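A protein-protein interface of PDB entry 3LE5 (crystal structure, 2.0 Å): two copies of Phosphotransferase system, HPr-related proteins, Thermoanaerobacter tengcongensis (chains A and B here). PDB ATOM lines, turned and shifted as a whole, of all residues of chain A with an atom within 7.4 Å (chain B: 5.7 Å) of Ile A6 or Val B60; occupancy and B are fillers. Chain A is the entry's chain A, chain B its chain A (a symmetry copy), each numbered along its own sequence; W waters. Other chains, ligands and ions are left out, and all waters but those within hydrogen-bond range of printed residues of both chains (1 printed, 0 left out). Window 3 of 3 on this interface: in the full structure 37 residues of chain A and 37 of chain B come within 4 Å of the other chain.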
ATOM      1  N   VAL A   4     -21.121 -13.965   5.957  1.00  0.00           N
ATOM      2  CA  VAL A   4     -22.137 -12.989   6.370  1.00  0.00           C
ATOM      3  C   VAL A   4     -23.171 -12.756   5.269  1.00  0.00           C
ATOM      4  O   VAL A   4     -22.809 -12.549   4.113  1.00  0.00           O
ATOM      5  CB  VAL A   4     -21.514 -11.631   6.755  1.00  0.00           C
ATOM      6  CG1 VAL A   4     -20.451 -11.821   7.803  1.00  0.00           C
ATOM      7  CG2 VAL A   4     -20.921 -10.942   5.541  1.00  0.00           C
ATOM      8  N   THR A   5     -24.458 -12.811   5.613  1.00  0.00           N
ATOM      9  CA  THR A   5     -25.484 -12.360   4.673  1.00  0.00           C
ATOM     10  C   THR A   5     -25.809 -10.917   4.998  1.00  0.00           C
ATOM     11  O   THR A   5     -26.226 -10.591   6.110  1.00  0.00           O
ATOM     12  CB  THR A   5     -26.782 -13.201   4.670  1.00  0.00           C
ATOM     13  OG1 THR A   5     -27.578 -12.873   5.813  1.00  0.00           O
ATOM     14  CG2 THR A   5     -26.480 -14.695   4.639  1.00  0.00           C
ATOM     15  N   ILE A   6     -25.595 -10.053   4.017  1.00  0.00           N
ATOM     16  CA  ILE A   6     -25.666  -8.624   4.243  1.00  0.00           C
ATOM     17  C   ILE A   6     -26.452  -7.957   3.131  1.00  0.00           C
ATOM     18  O   ILE A   6     -26.498  -8.452   2.000  1.00  0.00           O
ATOM     19  CB  ILE A   6     -24.258  -8.025   4.309  1.00  0.00           C
ATOM     20  CG1 ILE A   6     -24.323  -6.555   4.718  1.00  0.00           C
ATOM     21  CG2 ILE A   6     -23.547  -8.222   2.980  1.00  0.00           C
ATOM     22  CD1 ILE A   6     -22.967  -5.914   4.886  1.00  0.00           C
ATOM     23  N   GLU A   7     -27.079  -6.833   3.463  1.00  0.00           N
ATOM     24  CA  GLU A   7     -27.886  -6.097   2.507  1.00  0.00           C
ATOM     25  C   GLU A   7     -27.060  -5.017   1.828  1.00  0.00           C
ATOM     26  O   GLU A   7     -26.315  -4.286   2.485  1.00  0.00           O
ATOM     27  CB  GLU A   7     -29.083  -5.472   3.212  1.00  0.00           C
ATOM     28  CG  GLU A   7     -30.024  -4.735   2.295  1.00  0.00           C
ATOM     29  CD  GLU A   7     -31.282  -4.307   3.006  1.00  0.00           C
ATOM     30  OE1 GLU A   7     -31.365  -4.510   4.238  1.00  0.00           O
ATOM     31  OE2 GLU A   7     -32.189  -3.774   2.334  1.00  0.00           O
ATOM     32  N   ILE A   8     -27.192  -4.931   0.506  1.00  0.00           N
ATOM     33  CA  ILE A   8     -26.505  -3.914  -0.291  1.00  0.00           C
ATOM     34  C   ILE A   8     -27.346  -2.638  -0.365  1.00  0.00           C
ATOM     35  O   ILE A   8     -28.407  -2.630  -0.981  1.00  0.00           O
ATOM     36  CB  ILE A   8     -26.231  -4.434  -1.716  1.00  0.00           C
ATOM     37  CG1 ILE A   8     -25.542  -5.802  -1.654  1.00  0.00           C
ATOM     38  CG2 ILE A   8     -25.428  -3.416  -2.524  1.00  0.00           C
ATOM     39  CD1 ILE A   8     -24.203  -5.774  -0.953  1.00  0.00           C
ATOM     40  N   LYS A   9     -26.878  -1.559   0.257  1.00  0.00           N
ATOM     41  CA  LYS A   9     -27.730  -0.384   0.434  1.00  0.00           C
ATOM     42  C   LYS A   9     -27.346   0.843  -0.405  1.00  0.00           C
ATOM     43  O   LYS A   9     -28.085   1.824  -0.438  1.00  0.00           O
ATOM     44  CB  LYS A   9     -27.843  -0.032   1.925  1.00  0.00           C
ATOM     45  CG  LYS A   9     -28.514  -1.123   2.765  1.00  0.00           C
ATOM     46  CD  LYS A   9     -28.611  -0.756   4.248  1.00  0.00           C
ATOM     47  CE  LYS A   9     -29.482  -1.770   4.995  1.00  0.00           C
ATOM     48  NZ  LYS A   9     -29.786  -1.375   6.401  1.00  0.00           N
ATOM     49  N   GLU B  36     -22.482 -14.841  -3.086  1.00  0.00           N
ATOM     50  CA  GLU B  36     -23.593 -15.686  -3.462  1.00  0.00           C
ATOM     51  C   GLU B  36     -24.878 -14.875  -3.377  1.00  0.00           C
ATOM     52  O   GLU B  36     -25.249 -14.388  -2.312  1.00  0.00           O
ATOM     53  CB  GLU B  36     -23.637 -16.892  -2.521  1.00  0.00           C
ATOM     54  CG  GLU B  36     -24.708 -17.931  -2.813  1.00  0.00           C
ATOM     55  CD  GLU B  36     -24.738 -19.035  -1.759  1.00  0.00           C
ATOM     56  OE1 GLU B  36     -23.653 -19.383  -1.237  1.00  0.00           O
ATOM     57  OE2 GLU B  36     -25.840 -19.551  -1.449  1.00  0.00           O
ATOM     58  N   LYS B  37     -25.546 -14.705  -4.511  1.00  0.00           N
ATOM     59  CA  LYS B  37     -26.839 -14.035  -4.523  1.00  0.00           C
ATOM     60  C   LYS B  37     -27.885 -14.932  -5.153  1.00  0.00           C
ATOM     61  O   LYS B  37     -27.856 -15.163  -6.361  1.00  0.00           O
ATOM     62  CB  LYS B  37     -26.779 -12.714  -5.288  1.00  0.00           C
ATOM     63  CG  LYS B  37     -28.076 -11.937  -5.198  1.00  0.00           C
ATOM     64  CD  LYS B  37     -28.324 -11.115  -6.437  1.00  0.00           C
ATOM     65  CE  LYS B  37     -29.800 -10.790  -6.574  1.00  0.00           C
ATOM     66  NZ  LYS B  37     -30.096 -10.127  -7.871  1.00  0.00           N
ATOM     67  N   ASP B  38     -28.808 -15.430  -4.332  1.00  0.00           N
ATOM     68  CA  ASP B  38     -29.884 -16.305  -4.800  1.00  0.00           C
ATOM     69  C   ASP B  38     -29.319 -17.583  -5.408  1.00  0.00           C
ATOM     70  O   ASP B  38     -29.693 -17.978  -6.520  1.00  0.00           O
ATOM     71  CB  ASP B  38     -30.782 -15.582  -5.814  1.00  0.00           C
ATOM     72  N   GLY B  58     -30.487  -2.816  -2.071  1.00  0.00           N
ATOM     73  CA  GLY B  58     -31.554  -3.589  -1.451  1.00  0.00           C
ATOM     74  C   GLY B  58     -31.353  -5.102  -1.412  1.00  0.00           C
ATOM     75  O   GLY B  58     -31.999  -5.803  -0.621  1.00  0.00           O
ATOM     76  N   ASN B  59     -30.468  -5.612  -2.269  1.00  0.00           N
ATOM     77  CA  ASN B  59     -30.209  -7.048  -2.350  1.00  0.00           C
ATOM     78  C   ASN B  59     -29.438  -7.592  -1.154  1.00  0.00           C
ATOM     79  O   ASN B  59     -28.477  -6.980  -0.687  1.00  0.00           O
ATOM     80  CB  ASN B  59     -29.461  -7.391  -3.645  1.00  0.00           C
ATOM     81  CG  ASN B  59     -30.367  -7.986  -4.705  1.00  0.00           C
ATOM     82  OD1 ASN B  59     -30.257  -7.658  -5.888  1.00  0.00           O
ATOM     83  ND2 ASN B  59     -31.264  -8.875  -4.287  1.00  0.00           N
ATOM     84  N   VAL B  60     -29.866  -8.746  -0.660  1.00  0.00           N
ATOM     85  CA  VAL B  60     -29.091  -9.464   0.334  1.00  0.00           C
ATOM     86  C   VAL B  60     -28.283 -10.530  -0.376  1.00  0.00           C
ATOM     87  O   VAL B  60     -28.811 -11.304  -1.178  1.00  0.00           O
ATOM     88  CB  VAL B  60     -29.975 -10.121   1.394  1.00  0.00           C
ATOM     89  CG1 VAL B  60     -29.119 -10.922   2.347  1.00  0.00           C
ATOM     90  CG2 VAL B  60     -30.765  -9.067   2.148  1.00  0.00           C
ATOM     91  N   VAL B  61     -26.988 -10.545  -0.096  1.00  0.00           N
ATOM     92  CA  VAL B  61     -26.109 -11.575  -0.622  1.00  0.00           C
ATOM     93  C   VAL B  61     -25.376 -12.241   0.529  1.00  0.00           C
ATOM     94  O   VAL B  61     -25.324 -11.705   1.641  1.00  0.00           O
ATOM     95  CB  VAL B  61     -25.070 -11.004  -1.604  1.00  0.00           C
ATOM     96  CG1 VAL B  61     -25.758 -10.346  -2.795  1.00  0.00           C
ATOM     97  CG2 VAL B  61     -24.150 -10.023  -0.888  1.00  0.00           C
ATOM     98  N   LYS B  62     -24.815 -13.412   0.251  1.00  0.00           N
ATOM     99  CA  LYS B  62     -24.030 -14.148   1.225  1.00  0.00           C
ATOM    100  C   LYS B  62     -22.551 -13.960   0.903  1.00  0.00           C
ATOM    101  O   LYS B  62     -22.089 -14.343  -0.171  1.00  0.00           O
ATOM    102  CB  LYS B  62     -24.412 -15.628   1.191  1.00  0.00           C
ATOM    103  CG  LYS B  62     -24.121 -16.375   2.473  1.00  0.00           C
ATOM    104  CD  LYS B  62     -24.542 -17.834   2.373  1.00  0.00           C
ATOM    105  CE  LYS B  62     -23.538 -18.648   1.572  1.00  0.00           C
ATOM    106  NZ  LYS B  62     -23.762 -20.114   1.719  1.00  0.00           N
ATOM    107  N   LEU B  63     -21.824 -13.346   1.834  1.00  0.00           N
ATOM    108  CA  LEU B  63     -20.385 -13.094   1.701  1.00  0.00           C
ATOM    109  C   LEU B  63     -19.566 -14.133   2.451  1.00  0.00           C
ATOM    110  O   LEU B  63     -19.622 -14.184   3.677  1.00  0.00           O
ATOM    111  CB  LEU B  63     -20.032 -11.730   2.302  1.00  0.00           C
ATOM    112  CG  LEU B  63     -19.925 -10.487   1.433  1.00  0.00           C
ATOM    113  CD1 LEU B  63     -19.542  -9.323   2.318  1.00  0.00           C
ATOM    114  CD2 LEU B  63     -18.892 -10.708   0.344  1.00  0.00           C
ATOM    115  N   VAL B  78     -17.352  -6.012   4.436  1.00  0.00           N
ATOM    116  CA  VAL B  78     -18.552  -5.642   5.169  1.00  0.00           C
ATOM    117  C   VAL B  78     -18.524  -4.167   5.571  1.00  0.00           C
ATOM    118  O   VAL B  78     -19.504  -3.448   5.363  1.00  0.00           O
ATOM    119  CB  VAL B  78     -18.755  -6.538   6.409  1.00  0.00           C
ATOM    120  CG1 VAL B  78     -19.900  -6.017   7.255  1.00  0.00           C
ATOM    121  CG2 VAL B  78     -19.015  -7.975   5.982  1.00  0.00           C
ATOM    122  N   ILE B  81     -18.976  -2.050   2.521  1.00  0.00           N
ATOM    123  CA  ILE B  81     -20.385  -2.086   2.158  1.00  0.00           C
ATOM    124  C   ILE B  81     -21.222  -1.193   3.065  1.00  0.00           C
ATOM    125  O   ILE B  81     -22.107  -0.474   2.606  1.00  0.00           O
ATOM    126  CB  ILE B  81     -20.923  -3.527   2.256  1.00  0.00           C
ATOM    127  CG1 ILE B  81     -20.391  -4.366   1.095  1.00  0.00           C
ATOM    128  CG2 ILE B  81     -22.442  -3.543   2.281  1.00  0.00           C
ATOM    129  CD1 ILE B  81     -20.691  -5.835   1.218  1.00  0.00           C
ATOM    130  N   GLU B  82     -20.931  -1.243   4.357  1.00  0.00           N
ATOM    131  CA  GLU B  82     -21.738  -0.548   5.352  1.00  0.00           C
ATOM    132  C   GLU B  82     -21.684   0.981   5.255  1.00  0.00           C
ATOM    133  O   GLU B  82     -22.584   1.672   5.735  1.00  0.00           O
ATOM    134  CB  GLU B  82     -21.355  -1.007   6.764  1.00  0.00           C
ATOM    135  CG  GLU B  82     -21.770  -2.444   7.080  1.00  0.00           C
ATOM    136  CD  GLU B  82     -21.715  -2.771   8.568  1.00  0.00           C
ATOM    137  OE1 GLU B  82     -21.092  -1.996   9.332  1.00  0.00           O
ATOM    138  OE2 GLU B  82     -22.298  -3.806   8.970  1.00  0.00           O
HETATM  139  O   HOH W   1     -23.991  -0.539   0.226  1.00  0.00           O
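The backbone NH (N) of Leu B63 lies within hydrogen-bond range of the backbone carbonyl oxygen (O) of Val A4 (2.6 Å).
The backbone NH of Ile A6 lies within hydrogen-bond range of the backbone carbonyl oxygen of Val B61 (2.9 Å).
N of Ile A8 sits at hydrogen-bond distance from O of Asn B59 (2.7 Å).
The backbone NH of Gly B58 sits close to the backbone carbonyl oxygen of Ile A8.
The side-chain carboxylate (OE1) of Glu B36 is in salt-bridge range of the side-chain amino group (NZ) of Lys B62 (3.0 Å).
The side-chain amide oxygen of Asn B59 sits at hydrogen-bond distance from the side-chain amino group of Lys B37.
Among the printed residues, merely in contact across the chains: Thr A5 with Val B61 (3.1 Å), Ile A6 with Val B60 (3.2 Å), Glu A7 with Asn B59 (3.4 Å), Val A4 with Lys B62 (3.5 Å), Val A4 with Val B78 (3.6 Å), Ile A6 with Ile B81 (3.6 Å), Glu A7 with Gly B58 (3.6 Å), Thr A5 with Lys B62 (3.6 Å), Val A4 with Val B61 (3.6 Å), Ile A6 with Asn B59 (3.6 Å), Ile A6 with Val B78 (3.9 Å) and Glu A7 with Ile B81 (3.9 Å).
Of the printed residues of chain B, Ile A6 touches Asn B59 (3.6 Å), Val B60 (3.2 Å), Val B61 (2.9 Å), Val B78 (3.9 Å) and Ile B81 (3.6 Å).
Of the printed residues of chain A, Lys B62 touches Val A4 (3.5 Å) and Thr A5 (3.6 Å).
Printed residues of chain A within 4 Å of Leu B63: Val A4.
Printed residues of chain A within 4 Å of Asn B59: Ile A6, Glu A7 and Ile A8.
Of the printed residues of chain B, Ile A8 touches Gly B58 and Asn B59.
Of the printed residues of chain B, Glu A7 touches Gly B58 (3.6 Å), Asn B59 (3.4 Å) and Ile B81 (3.9 Å).
Asp B38 touches none of the printed residues of chain A.
The nearest printed residue of chain A that does not touch Val B60 is Thr A5 (4.01 Å).
The nearest printed residue of chain A that does not touch Val B61 is Ile A8 (4.2 Å).
Hydrophobic or aromatic side chains of chain B within 4 Å of the printed part of chain A: Val B60, Leu B63, Val B78 and Ile B81.
Among the printed residues, 16 pairs touch across the chains.
Among the printed residues, no Asp or Glu carboxylate lies within 4 Å of a Lys or Arg side-chain nitrogen of the other chain.
No position is printed for both chains.
Of the 16 pairs that touch across the chains among the printed residues, none has its exchanged pair printed and touching as well.
Water W1 bridges O of Ile B81 and N of Lys A9.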
